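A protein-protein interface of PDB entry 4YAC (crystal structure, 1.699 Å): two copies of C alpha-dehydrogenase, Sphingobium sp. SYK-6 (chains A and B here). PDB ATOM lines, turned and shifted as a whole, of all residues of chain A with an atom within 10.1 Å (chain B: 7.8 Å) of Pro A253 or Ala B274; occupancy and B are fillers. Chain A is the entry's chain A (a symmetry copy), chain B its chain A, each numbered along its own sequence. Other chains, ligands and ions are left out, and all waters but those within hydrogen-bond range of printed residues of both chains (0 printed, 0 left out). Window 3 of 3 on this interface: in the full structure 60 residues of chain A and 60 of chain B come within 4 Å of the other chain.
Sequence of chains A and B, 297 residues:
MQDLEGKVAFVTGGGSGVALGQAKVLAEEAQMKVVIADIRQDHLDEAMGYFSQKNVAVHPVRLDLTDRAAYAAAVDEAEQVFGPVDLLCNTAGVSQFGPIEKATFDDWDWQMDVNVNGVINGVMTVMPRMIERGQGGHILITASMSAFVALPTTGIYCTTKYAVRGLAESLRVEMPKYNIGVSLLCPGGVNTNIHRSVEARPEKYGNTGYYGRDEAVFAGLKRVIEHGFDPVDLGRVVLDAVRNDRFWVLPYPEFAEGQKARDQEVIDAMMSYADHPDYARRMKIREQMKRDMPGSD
No position is printed for both chains. Of the 24 pairs that touch across the chains among the printed residues, none has its exchanged pair printed and touching as well.
Among the printed residues, pairs that only touch across the chains: Leu A221 with Arg B286 (3.2 Å), Leu A250 with Met B270 (3.4 Å), Pro A253 with Tyr B279 (3.4 Å), Pro A251 with Tyr B273 (3.5 Å), Pro A251 with Arg B282 (3.5 Å), Pro A253 with Ala B274 (3.6 Å), Ala A256 with Ile B267 (3.6 Å), Pro A253 with Tyr B273 (3.6 Å), Pro A253 with Arg B282 (3.6 Å), Ala A256 with Met B271 (3.6 Å), Glu A254 with Tyr B279 (3.7 Å), Tyr A252 with Met B270 (3.8 Å), Val A249 with Tyr B273 (3.8 Å), Phe A255 with Met B270 (3.8 Å), Gln A259 with Ile B267 (3.8 Å), Lys A260 with Ile B267 (3.8 Å), Pro A253 with Met B271 (3.8 Å), Leu A250 with Tyr B273 (3.9 Å), Met A145 with Met B270 (3.9 Å) and Leu A250 with Ala B269 (3.98 Å).
Of the 18 printed residues of chain B, 9 touch a printed residue of chain A. Printed residues of chain B that touch a printed residue of chain A: Ile B267, Ala B269, Met B270, Met B271, Tyr B273, Ala B274, Tyr B279, Arg B282 and Arg B286. Hydrophobic or aromatic side chains of chain B within 4 Å of the printed part of chain A: Ile B267, Met B270, Met B271, Tyr B273 and Tyr B279. Hydrophobic or aromatic side chains of chain A that line the printed part of chain B: Met A145, Leu A221, Val A249, Leu A250, Pro A251, Pro A253 and Ala A256. Along chain A the printed residues that touch a printed residue of chain B span positions 145 to 260. Among the printed residues, 24 pairs touch across the chains.
SD of Met B270 lies within hydrogen-bond range of N of Ala A256, at 3.8 Å. The side-chain carboxylate (OE2) of Glu A254 lies within salt-bridge range of the guanidinium group (NE) of Arg B282, 2.5 Å away. The side-chain carboxylate (OE2) of Glu A254 is in salt-bridge range of the guanidinium group (NH2) of Arg B286, 3.5 Å away. The backbone nitrogen (N) of Pro A253 lies close to the backbone carbonyl oxygen (O) of Met B270 (3.5 Å).
Of the printed residues of chain B, Pro A253 touches Met B270, Met B271, Tyr B273, Ala B274, Tyr B279 and Arg B282. Of the printed residues of chain B, Glu A254 touches Tyr B279, Arg B282 and Arg B286. Of chain A, only Pro A253 (3.8 Å) and Ala A256 (3.6 Å) come within 4 Å of Met B271. No residue of chain A comes within 4 Å of Ser B272. Of the printed residues of chain A, Tyr B273 touches Val A249 (3.8 Å), Leu A250 (3.9 Å), Pro A251 (3.5 Å) and Pro A253 (3.6 Å). Of chain A, only Pro A253 (3.6 Å) comes within 4 Å of Ala B274. No residue of chain A comes within 4 Å of Asp B275. Tyr B279 touches just these residues of chain A: Pro A253 and Glu A254. The nearest residue of chain B that does not touch Pro A253 is Ser B272 (5.6 Å).
O of Ala B269 is in hydrogen-bond range of OG of Ser B272, at 2.6 Å. The side-chain hydroxyl (OH) of Tyr B279 lies close to the side-chain sulfur (SD) of Met B283 (3.6 Å). The side-chain amino group (NZ) of Lys A260 is in salt-bridge range of the side-chain carboxylate (OE2) of Glu A257.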
ATOM      1  N   MET A 145       6.165 -18.893  17.154  1.00  0.00           N
ATOM      2  CA  MET A 145       6.787 -19.927  16.338  1.00  0.00           C
ATOM      3  C   MET A 145       8.101 -20.379  16.975  1.00  0.00           C
ATOM      4  O   MET A 145       8.674 -21.391  16.574  1.00  0.00           O
ATOM      5  CB  MET A 145       7.019 -19.433  14.910  1.00  0.00           C
ATOM      6  CG  MET A 145       5.771 -19.463  14.039  1.00  0.00           C
ATOM      7  SD  MET A 145       4.998 -21.095  13.935  1.00  0.00           S
ATOM      8  CE  MET A 145       6.347 -22.099  13.314  1.00  0.00           C
ATOM      9  N   CYS A 186       0.495 -19.188  17.565  1.00  0.00           N
ATOM     10  CA  CYS A 186       1.943 -19.058  17.436  1.00  0.00           C
ATOM     11  C   CYS A 186       2.303 -18.025  16.376  1.00  0.00           C
ATOM     12  O   CYS A 186       2.535 -18.380  15.219  1.00  0.00           O
ATOM     13  CB  CYS A 186       2.576 -20.403  17.080  1.00  0.00           C
ATOM     14  SG  CYS A 186       2.408 -21.657  18.368  1.00  0.00           S
ATOM     15  N   PHE A 218      14.285 -19.535   7.464  1.00  0.00           N
ATOM     16  CA  PHE A 218      13.224 -19.324   8.441  1.00  0.00           C
ATOM     17  C   PHE A 218      13.101 -17.846   8.787  1.00  0.00           C
ATOM     18  O   PHE A 218      12.002 -17.294   8.808  1.00  0.00           O
ATOM     19  CB  PHE A 218      13.467 -20.126   9.720  1.00  0.00           C
ATOM     20  CG  PHE A 218      12.427 -19.884  10.780  1.00  0.00           C
ATOM     21  CD1 PHE A 218      12.676 -19.024  11.837  1.00  0.00           C
ATOM     22  CD2 PHE A 218      11.187 -20.497  10.700  1.00  0.00           C
ATOM     23  CE1 PHE A 218      11.713 -18.794  12.805  1.00  0.00           C
ATOM     24  CE2 PHE A 218      10.220 -20.269  11.665  1.00  0.00           C
ATOM     25  CZ  PHE A 218      10.485 -19.417  12.719  1.00  0.00           C
ATOM     26  N   LEU A 221      11.558 -15.966   5.844  1.00  0.00           N
ATOM     27  CA  LEU A 221      10.118 -16.166   5.783  1.00  0.00           C
ATOM     28  C   LEU A 221       9.467 -15.372   6.902  1.00  0.00           C
ATOM     29  O   LEU A 221       8.435 -14.736   6.706  1.00  0.00           O
ATOM     30  CB  LEU A 221       9.766 -17.650   5.896  1.00  0.00           C
ATOM     31  CG  LEU A 221      10.281 -18.541   4.761  1.00  0.00           C
ATOM     32  CD1 LEU A 221       9.884 -19.992   4.989  1.00  0.00           C
ATOM     33  CD2 LEU A 221       9.781 -18.049   3.412  1.00  0.00           C
ATOM     34  N   ILE A 225       6.419 -12.096   6.972  1.00  0.00           N
ATOM     35  CA  ILE A 225       5.175 -12.039   7.751  1.00  0.00           C
ATOM     36  C   ILE A 225       5.246 -10.857   8.715  1.00  0.00           C
ATOM     37  O   ILE A 225       4.249 -10.156   8.897  1.00  0.00           O
ATOM     38  CB  ILE A 225       4.847 -13.393   8.531  1.00  0.00           C
ATOM     39  CG1 ILE A 225       3.981 -13.157   9.796  1.00  0.00           C
ATOM     40  CG2 ILE A 225       6.101 -14.207   8.847  1.00  0.00           C
ATOM     41  CD1 ILE A 225       4.406 -13.930  11.031  1.00  0.00           C
ATOM     42  N   VAL A 249      -3.340 -22.843  15.943  1.00  0.00           N
ATOM     43  CA  VAL A 249      -3.506 -21.594  15.208  1.00  0.00           C
ATOM     44  C   VAL A 249      -2.131 -21.137  14.731  1.00  0.00           C
ATOM     45  O   VAL A 249      -1.451 -20.348  15.390  1.00  0.00           O
ATOM     46  CB  VAL A 249      -4.187 -20.504  16.060  1.00  0.00           C
ATOM     47  CG1 VAL A 249      -4.624 -19.342  15.178  1.00  0.00           C
ATOM     48  CG2 VAL A 249      -5.393 -21.082  16.795  1.00  0.00           C
ATOM     49  N   LEU A 250      -1.744 -21.664  13.574  1.00  0.00           N
ATOM     50  CA  LEU A 250      -0.436 -21.433  12.973  1.00  0.00           C
ATOM     51  C   LEU A 250      -0.632 -20.930  11.545  1.00  0.00           C
ATOM     52  O   LEU A 250      -0.459 -21.683  10.591  1.00  0.00           O
ATOM     53  CB  LEU A 250       0.391 -22.725  12.970  1.00  0.00           C
ATOM     54  CG  LEU A 250       0.324 -23.624  14.207  1.00  0.00           C
ATOM     55  CD1 LEU A 250       0.814 -25.020  13.867  1.00  0.00           C
ATOM     56  CD2 LEU A 250       1.134 -23.041  15.337  1.00  0.00           C
ATOM     57  N   PRO A 251      -1.002 -19.654  11.388  1.00  0.00           N
ATOM     58  CA  PRO A 251      -1.452 -19.207  10.065  1.00  0.00           C
ATOM     59  C   PRO A 251      -0.317 -18.890   9.083  1.00  0.00           C
ATOM     60  O   PRO A 251      -0.357 -17.863   8.406  1.00  0.00           O
ATOM     61  CB  PRO A 251      -2.274 -17.958  10.398  1.00  0.00           C
ATOM     62  CG  PRO A 251      -1.641 -17.407  11.618  1.00  0.00           C
ATOM     63  CD  PRO A 251      -1.104 -18.584  12.397  1.00  0.00           C
ATOM     64  N   TYR A 252       0.665 -19.784   8.990  1.00  0.00           N
ATOM     65  CA  TYR A 252       1.817 -19.582   8.113  1.00  0.00           C
ATOM     66  C   TYR A 252       2.191 -20.860   7.366  1.00  0.00           C
ATOM     67  O   TYR A 252       3.035 -21.628   7.830  1.00  0.00           O
ATOM     68  CB  TYR A 252       3.014 -19.080   8.923  1.00  0.00           C
ATOM     69  CG  TYR A 252       2.645 -17.973   9.875  1.00  0.00           C
ATOM     70  CD1 TYR A 252       2.230 -16.738   9.401  1.00  0.00           C
ATOM     71  CD2 TYR A 252       2.696 -18.165  11.247  1.00  0.00           C
ATOM     72  CE1 TYR A 252       1.877 -15.728  10.264  1.00  0.00           C
ATOM     73  CE2 TYR A 252       2.350 -17.155  12.120  1.00  0.00           C
ATOM     74  CZ  TYR A 252       1.943 -15.937  11.621  1.00  0.00           C
ATOM     75  OH  TYR A 252       1.596 -14.920  12.475  1.00  0.00           O
ATOM     76  N   PRO A 253       1.567 -21.091   6.198  1.00  0.00           N
ATOM     77  CA  PRO A 253       1.864 -22.293   5.407  1.00  0.00           C
ATOM     78  C   PRO A 253       3.324 -22.358   4.953  1.00  0.00           C
ATOM     79  O   PRO A 253       3.788 -23.421   4.541  1.00  0.00           O
ATOM     80  CB  PRO A 253       0.922 -22.174   4.203  1.00  0.00           C
ATOM     81  CG  PRO A 253      -0.118 -21.185   4.599  1.00  0.00           C
ATOM     82  CD  PRO A 253       0.519 -20.262   5.577  1.00  0.00           C
ATOM     83  N   GLU A 254       4.032 -21.234   5.030  1.00  0.00           N
ATOM     84  CA  GLU A 254       5.448 -21.181   4.669  1.00  0.00           C
ATOM     85  C   GLU A 254       6.284 -22.158   5.475  1.00  0.00           C
ATOM     86  O   GLU A 254       7.150 -22.849   4.939  1.00  0.00           O
ATOM     87  CB  GLU A 254       6.017 -19.785   4.897  1.00  0.00           C
ATOM     88  CG  GLU A 254       5.251 -18.672   4.269  1.00  0.00           C
ATOM     89  CD  GLU A 254       4.250 -18.031   5.206  1.00  0.00           C
ATOM     90  OE1 GLU A 254       3.323 -18.729   5.655  1.00  0.00           O
ATOM     91  OE2 GLU A 254       4.402 -16.826   5.494  1.00  0.00           O
ATOM     92  N   PHE A 255       6.024 -22.187   6.776  1.00  0.00           N
ATOM     93  CA  PHE A 255       6.857 -22.919   7.717  1.00  0.00           C
ATOM     94  C   PHE A 255       6.678 -24.431   7.596  1.00  0.00           C
ATOM     95  O   PHE A 255       7.363 -25.195   8.274  1.00  0.00           O
ATOM     96  CB  PHE A 255       6.542 -22.457   9.145  1.00  0.00           C
ATOM     97  CG  PHE A 255       6.858 -21.001   9.398  1.00  0.00           C
ATOM     98  CD1 PHE A 255       7.979 -20.410   8.835  1.00  0.00           C
ATOM     99  CD2 PHE A 255       6.033 -20.223  10.196  1.00  0.00           C
ATOM    100  CE1 PHE A 255       8.272 -19.078   9.063  1.00  0.00           C
ATOM    101  CE2 PHE A 255       6.322 -18.888  10.428  1.00  0.00           C
ATOM    102  CZ  PHE A 255       7.442 -18.318   9.861  1.00  0.00           C
ATOM    103  N   ALA A 256       5.768 -24.856   6.721  1.00  0.00           N
ATOM    104  CA  ALA A 256       5.448 -26.272   6.567  1.00  0.00           C
ATOM    105  C   ALA A 256       6.667 -27.107   6.174  1.00  0.00           C
ATOM    106  O   ALA A 256       7.040 -28.032   6.893  1.00  0.00           O
ATOM    107  CB  ALA A 256       4.343 -26.447   5.538  1.00  0.00           C
ATOM    108  N   GLU A 257       7.281 -26.785   5.040  1.00  0.00           N
ATOM    109  CA  GLU A 257       8.403 -27.576   4.540  1.00  0.00           C
ATOM    110  C   GLU A 257       9.565 -27.545   5.527  1.00  0.00           C
ATOM    111  O   GLU A 257      10.238 -28.555   5.732  1.00  0.00           O
ATOM    112  CB  GLU A 257       8.862 -27.075   3.166  1.00  0.00           C
ATOM    113  CG  GLU A 257       7.868 -27.322   2.026  1.00  0.00           C
ATOM    114  CD  GLU A 257       7.417 -28.770   1.926  1.00  0.00           C
ATOM    115  OE1 GLU A 257       8.277 -29.652   1.722  1.00  0.00           O
ATOM    116  OE2 GLU A 257       6.198 -29.028   2.048  1.00  0.00           O
ATOM    117  N   GLY A 258       9.794 -26.391   6.141  1.00  0.00           N
ATOM    118  CA  GLY A 258      10.823 -26.273   7.157  1.00  0.00           C
ATOM    119  C   GLY A 258      10.503 -27.122   8.375  1.00  0.00           C
ATOM    120  O   GLY A 258      11.392 -27.735   8.966  1.00  0.00           O
ATOM    121  N   GLN A 259       9.228 -27.159   8.751  1.00  0.00           N
ATOM    122  CA  GLN A 259       8.796 -27.932   9.909  1.00  0.00           C
ATOM    123  C   GLN A 259       8.846 -29.431   9.606  1.00  0.00           C
ATOM    124  O   GLN A 259       9.154 -30.237  10.485  1.00  0.00           O
ATOM    125  CB  GLN A 259       7.384 -27.517  10.342  1.00  0.00           C
ATOM    126  CG  GLN A 259       6.928 -28.125  11.663  1.00  0.00           C
ATOM    127  CD  GLN A 259       7.877 -27.815  12.811  1.00  0.00           C
ATOM    128  OE1 GLN A 259       8.302 -26.672  12.991  1.00  0.00           O
ATOM    129  NE2 GLN A 259       8.225 -28.838  13.583  1.00  0.00           N
ATOM    130  N   LYS A 260       8.551 -29.799   8.362  1.00  0.00           N
ATOM    131  CA  LYS A 260       8.633 -31.195   7.937  1.00  0.00           C
ATOM    132  C   LYS A 260      10.040 -31.737   8.129  1.00  0.00           C
ATOM    133  O   LYS A 260      10.228 -32.894   8.506  1.00  0.00           O
ATOM    134  CB  LYS A 260       8.239 -31.348   6.468  1.00  0.00           C
ATOM    135  CG  LYS A 260       6.754 -31.238   6.167  1.00  0.00           C
ATOM    136  CD  LYS A 260       6.524 -31.414   4.674  1.00  0.00           C
ATOM    137  CE  LYS A 260       5.056 -31.429   4.304  1.00  0.00           C
ATOM    138  NZ  LYS A 260       4.888 -31.774   2.864  1.00  0.00           N
ATOM    139  N   ARG A 262      12.359 -30.526  10.283  1.00  0.00           N
ATOM    140  CA  ARG A 262      12.574 -30.634  11.718  1.00  0.00           C
ATOM    141  C   ARG A 262      11.910 -31.897  12.257  1.00  0.00           C
ATOM    142  O   ARG A 262      12.492 -32.613  13.070  1.00  0.00           O
ATOM    143  CB  ARG A 262      12.036 -29.396  12.438  1.00  0.00           C
ATOM    144  CG  ARG A 262      12.898 -28.154  12.258  1.00  0.00           C
ATOM    145  CD  ARG A 262      12.402 -27.000  13.121  1.00  0.00           C
ATOM    146  NE  ARG A 262      11.142 -26.445  12.631  1.00  0.00           N
ATOM    147  CZ  ARG A 262      11.045 -25.512  11.687  1.00  0.00           C
ATOM    148  NH1 ARG A 262      12.134 -25.016  11.115  1.00  0.00           N
ATOM    149  NH2 ARG A 262       9.851 -25.071  11.316  1.00  0.00           N
ATOM    150  N   ILE B 267       1.455 -29.670  10.510  1.00  0.00           N
ATOM    151  CA  ILE B 267       1.624 -29.386   9.089  1.00  0.00           C
ATOM    152  C   ILE B 267       0.280 -29.048   8.446  1.00  0.00           C
ATOM    153  O   ILE B 267       0.169 -28.070   7.706  1.00  0.00           O
ATOM    154  CB  ILE B 267       2.268 -30.584   8.346  1.00  0.00           C
ATOM    155  CG1 ILE B 267       3.645 -30.913   8.936  1.00  0.00           C
ATOM    156  CG2 ILE B 267       2.385 -30.309   6.844  1.00  0.00           C
ATOM    157  CD1 ILE B 267       4.624 -29.749   8.955  1.00  0.00           C
ATOM    158  N   ASP B 268      -0.740 -29.850   8.739  1.00  0.00           N
ATOM    159  CA  ASP B 268      -2.068 -29.626   8.180  1.00  0.00           C
ATOM    160  C   ASP B 268      -2.639 -28.288   8.638  1.00  0.00           C
ATOM    161  O   ASP B 268      -3.304 -27.596   7.867  1.00  0.00           O
ATOM    162  CB  ASP B 268      -3.022 -30.761   8.566  1.00  0.00           C
ATOM    163  CG  ASP B 268      -2.715 -32.059   7.836  1.00  0.00           C
ATOM    164  OD1 ASP B 268      -1.934 -32.029   6.864  1.00  0.00           O
ATOM    165  OD2 ASP B 268      -3.263 -33.108   8.231  1.00  0.00           O
ATOM    166  N   ALA B 269      -2.376 -27.926   9.889  1.00  0.00           N
ATOM    167  CA  ALA B 269      -2.865 -26.664  10.432  1.00  0.00           C
ATOM    168  C   ALA B 269      -2.231 -25.489   9.698  1.00  0.00           C
ATOM    169  O   ALA B 269      -2.919 -24.542   9.316  1.00  0.00           O
ATOM    170  CB  ALA B 269      -2.580 -26.577  11.916  1.00  0.00           C
ATOM    171  N   MET B 270      -0.917 -25.558   9.505  1.00  0.00           N
ATOM    172  CA  MET B 270      -0.208 -24.541   8.740  1.00  0.00           C
ATOM    173  C   MET B 270      -0.757 -24.456   7.320  1.00  0.00           C
ATOM    174  O   MET B 270      -1.015 -23.369   6.807  1.00  0.00           O
ATOM    175  CB  MET B 270       1.291 -24.839   8.689  1.00  0.00           C
ATOM    176  CG  MET B 270       1.996 -24.795  10.029  1.00  0.00           C
ATOM    177  SD  MET B 270       3.735 -25.223   9.852  1.00  0.00           S
ATOM    178  CE  MET B 270       4.333 -24.954  11.519  1.00  0.00           C
ATOM    179  N   MET B 271      -0.936 -25.612   6.692  1.00  0.00           N
ATOM    180  CA  MET B 271      -1.380 -25.661   5.305  1.00  0.00           C
ATOM    181  C   MET B 271      -2.860 -25.304   5.150  1.00  0.00           C
ATOM    182  O   MET B 271      -3.320 -25.029   4.042  1.00  0.00           O
ATOM    183  CB  MET B 271      -1.123 -27.052   4.715  1.00  0.00           C
ATOM    184  CG  MET B 271       0.350 -27.400   4.495  1.00  0.00           C
ATOM    185  SD  MET B 271       1.284 -26.158   3.574  1.00  0.00           S
ATOM    186  CE  MET B 271       0.223 -25.901   2.155  1.00  0.00           C
ATOM    187  N   SER B 272      -3.605 -25.299   6.253  1.00  0.00           N
ATOM    188  CA  SER B 272      -5.035 -25.002   6.192  1.00  0.00           C
ATOM    189  C   SER B 272      -5.285 -23.524   5.892  1.00  0.00           C
ATOM    190  O   SER B 272      -6.396 -23.140   5.527  1.00  0.00           O
ATOM    191  CB  SER B 272      -5.727 -25.394   7.500  1.00  0.00           C
ATOM    192  OG  SER B 272      -5.424 -24.479   8.538  1.00  0.00           O
ATOM    193  N   TYR B 273      -4.250 -22.702   6.049  1.00  0.00           N
ATOM    194  CA  TYR B 273      -4.331 -21.282   5.715  1.00  0.00           C
ATOM    195  C   TYR B 273      -3.719 -20.994   4.342  1.00  0.00           C
ATOM    196  O   TYR B 273      -3.480 -19.839   3.995  1.00  0.00           O
ATOM    197  CB  TYR B 273      -3.619 -20.439   6.776  1.00  0.00           C
ATOM    198  CG  TYR B 273      -4.292 -20.412   8.132  1.00  0.00           C
ATOM    199  CD1 TYR B 273      -5.157 -19.383   8.477  1.00  0.00           C
ATOM    200  CD2 TYR B 273      -4.048 -21.405   9.072  1.00  0.00           C
ATOM    201  CE1 TYR B 273      -5.767 -19.345   9.717  1.00  0.00           C
ATOM    202  CE2 TYR B 273      -4.651 -21.375  10.318  1.00  0.00           C
ATOM    203  CZ  TYR B 273      -5.510 -20.342  10.635  1.00  0.00           C
ATOM    204  OH  TYR B 273      -6.116 -20.307  11.870  1.00  0.00           O
ATOM    205  N   ALA B 274      -3.461 -22.045   3.568  1.00  0.00           N
ATOM    206  CA  ALA B 274      -2.832 -21.897   2.255  1.00  0.00           C
ATOM    207  C   ALA B 274      -3.706 -21.098   1.289  1.00  0.00           C
ATOM    208  O   ALA B 274      -3.295 -20.051   0.785  1.00  0.00           O
ATOM    209  CB  ALA B 274      -2.522 -23.266   1.668  1.00  0.00           C
ATOM    210  N   ASP B 275      -4.913 -21.598   1.042  1.00  0.00           N
ATOM    211  CA  ASP B 275      -5.853 -20.973   0.114  1.00  0.00           C
ATOM    212  C   ASP B 275      -6.271 -19.565   0.544  1.00  0.00           C
ATOM    213  O   ASP B 275      -6.911 -18.838  -0.218  1.00  0.00           O
ATOM    214  CB  ASP B 275      -7.098 -21.851  -0.026  1.00  0.00           C
ATOM    215  CG  ASP B 275      -7.838 -22.022   1.288  1.00  0.00           C
ATOM    216  OD1 ASP B 275      -8.819 -21.285   1.522  1.00  0.00           O
ATOM    217  OD2 ASP B 275      -7.432 -22.889   2.093  1.00  0.00           O
ATOM    218  N   HIS B 276      -5.910 -19.192   1.767  1.00  0.00           N
ATOM    219  CA  HIS B 276      -6.269 -17.898   2.339  1.00  0.00           C
ATOM    220  C   HIS B 276      -5.354 -16.800   1.764  1.00  0.00           C
ATOM    221  O   HIS B 276      -4.153 -16.807   2.030  1.00  0.00           O
ATOM    222  CB  HIS B 276      -6.171 -17.982   3.868  1.00  0.00           C
ATOM    223  CG  HIS B 276      -6.561 -16.726   4.585  1.00  0.00           C
ATOM    224  ND1 HIS B 276      -7.503 -15.848   4.098  1.00  0.00           N
ATOM    225  CD2 HIS B 276      -6.144 -16.218   5.769  1.00  0.00           C
ATOM    226  CE1 HIS B 276      -7.641 -14.842   4.945  1.00  0.00           C
ATOM    227  NE2 HIS B 276      -6.831 -15.041   5.966  1.00  0.00           N
ATOM    228  N   PRO B 277      -5.917 -15.857   0.974  1.00  0.00           N
ATOM    229  CA  PRO B 277      -5.139 -14.962   0.097  1.00  0.00           C
ATOM    230  C   PRO B 277      -3.933 -14.239   0.705  1.00  0.00           C
ATOM    231  O   PRO B 277      -3.093 -13.777  -0.065  1.00  0.00           O
ATOM    232  CB  PRO B 277      -6.180 -13.923  -0.358  1.00  0.00           C
ATOM    233  CG  PRO B 277      -7.368 -14.117   0.518  1.00  0.00           C
ATOM    234  CD  PRO B 277      -7.357 -15.558   0.876  1.00  0.00           C
ATOM    235  N   ASP B 278      -3.838 -14.130   2.027  1.00  0.00           N
ATOM    236  CA  ASP B 278      -2.693 -13.455   2.636  1.00  0.00           C
ATOM    237  C   ASP B 278      -1.412 -14.234   2.350  1.00  0.00           C
ATOM    238  O   ASP B 278      -0.346 -13.651   2.154  1.00  0.00           O
ATOM    239  CB  ASP B 278      -2.886 -13.292   4.144  1.00  0.00           C
ATOM    240  CG  ASP B 278      -4.109 -12.466   4.490  1.00  0.00           C
ATOM    241  OD1 ASP B 278      -4.630 -11.765   3.597  1.00  0.00           O
ATOM    242  OD2 ASP B 278      -4.545 -12.511   5.661  1.00  0.00           O
ATOM    243  N   TYR B 279      -1.531 -15.556   2.328  1.00  0.00           N
ATOM    244  CA  TYR B 279      -0.416 -16.431   1.991  1.00  0.00           C
ATOM    245  C   TYR B 279       0.033 -16.213   0.549  1.00  0.00           C
ATOM    246  O   TYR B 279       1.228 -16.139   0.265  1.00  0.00           O
ATOM    247  CB  TYR B 279      -0.813 -17.892   2.207  1.00  0.00           C
ATOM    248  CG  TYR B 279       0.215 -18.892   1.739  1.00  0.00           C
ATOM    249  CD1 TYR B 279       1.424 -19.036   2.405  1.00  0.00           C
ATOM    250  CD2 TYR B 279      -0.026 -19.702   0.636  1.00  0.00           C
ATOM    251  CE1 TYR B 279       2.364 -19.952   1.985  1.00  0.00           C
ATOM    252  CE2 TYR B 279       0.910 -20.622   0.208  1.00  0.00           C
ATOM    253  CZ  TYR B 279       2.103 -20.744   0.887  1.00  0.00           C
ATOM    254  OH  TYR B 279       3.041 -21.658   0.466  1.00  0.00           O
ATOM    255  N   ALA B 280      -0.937 -16.110  -0.356  1.00  0.00           N
ATOM    256  CA  ALA B 280      -0.651 -15.888  -1.770  1.00  0.00           C
ATOM    257  C   ALA B 280       0.052 -14.551  -1.991  1.00  0.00           C
ATOM    258  O   ALA B 280       0.845 -14.408  -2.920  1.00  0.00           O
ATOM    259  CB  ALA B 280      -1.933 -15.953  -2.580  1.00  0.00           C
ATOM    260  N   ARG B 281      -0.249 -13.573  -1.143  1.00  0.00           N
ATOM    261  CA  ARG B 281       0.441 -12.289  -1.187  1.00  0.00           C
ATOM    262  C   ARG B 281       1.898 -12.460  -0.778  1.00  0.00           C
ATOM    263  O   ARG B 281       2.805 -12.002  -1.473  1.00  0.00           O
ATOM    264  CB  ARG B 281      -0.236 -11.269  -0.270  1.00  0.00           C
ATOM    265  CG  ARG B 281      -1.643 -10.888  -0.694  1.00  0.00           C
ATOM    266  CD  ARG B 281      -2.378 -10.143   0.411  1.00  0.00           C
ATOM    267  NE  ARG B 281      -2.098  -8.707   0.388  1.00  0.00           N
ATOM    268  CZ  ARG B 281      -3.021  -7.746   0.452  1.00  0.00           C
ATOM    269  NH1 ARG B 281      -4.312  -8.041   0.550  1.00  0.00           N
ATOM    270  NH2 ARG B 281      -2.646  -6.473   0.422  1.00  0.00           N
ATOM    271  N   ARG B 282       2.118 -13.123   0.354  1.00  0.00           N
ATOM    272  CA  ARG B 282       3.469 -13.336   0.854  1.00  0.00           C
ATOM    273  C   ARG B 282       4.288 -14.181  -0.129  1.00  0.00           C
ATOM    274  O   ARG B 282       5.496 -13.982  -0.261  1.00  0.00           O
ATOM    275  CB  ARG B 282       3.437 -13.996   2.236  1.00  0.00           C
ATOM    276  CG  ARG B 282       2.808 -13.146   3.327  1.00  0.00           C
ATOM    277  CD  ARG B 282       3.146 -13.690   4.709  1.00  0.00           C
ATOM    278  NE  ARG B 282       2.689 -15.066   4.890  1.00  0.00           N
ATOM    279  CZ  ARG B 282       1.465 -15.411   5.282  1.00  0.00           C
ATOM    280  NH1 ARG B 282       0.550 -14.483   5.535  1.00  0.00           N
ATOM    281  NH2 ARG B 282       1.151 -16.691   5.418  1.00  0.00           N
ATOM    282  N   MET B 283       3.629 -15.116  -0.815  1.00  0.00           N
ATOM    283  CA  MET B 283       4.254 -15.855  -1.914  1.00  0.00           C
ATOM    284  C   MET B 283       4.847 -14.902  -2.943  1.00  0.00           C
ATOM    285  O   MET B 283       6.021 -15.001  -3.306  1.00  0.00           O
ATOM    286  CB  MET B 283       3.238 -16.768  -2.616  1.00  0.00           C
ATOM    287  CG  MET B 283       2.932 -18.093  -1.933  1.00  0.00           C
ATOM    288  SD  MET B 283       4.362 -19.173  -1.752  1.00  0.00           S
ATOM    289  CE  MET B 283       4.867 -18.751  -0.096  1.00  0.00           C
ATOM    290  N   ARG B 286       8.155 -12.838  -2.194  1.00  0.00           N
ATOM    291  CA  ARG B 286       9.414 -13.574  -2.216  1.00  0.00           C
ATOM    292  C   ARG B 286       9.823 -13.942  -3.634  1.00  0.00           C
ATOM    293  O   ARG B 286      10.996 -13.837  -3.991  1.00  0.00           O
ATOM    294  CB  ARG B 286       9.307 -14.832  -1.360  1.00  0.00           C
ATOM    295  CG  ARG B 286       8.950 -14.524   0.071  1.00  0.00           C
ATOM    296  CD  ARG B 286       8.674 -15.774   0.863  1.00  0.00           C
ATOM    297  NE  ARG B 286       7.304 -15.741   1.346  1.00  0.00           N
ATOM    298  CZ  ARG B 286       6.604 -16.803   1.718  1.00  0.00           C
ATOM    299  NH1 ARG B 286       7.135 -18.018   1.667  1.00  0.00           N
ATOM    300  NH2 ARG B 286       5.355 -16.641   2.125  1.00  0.00           N
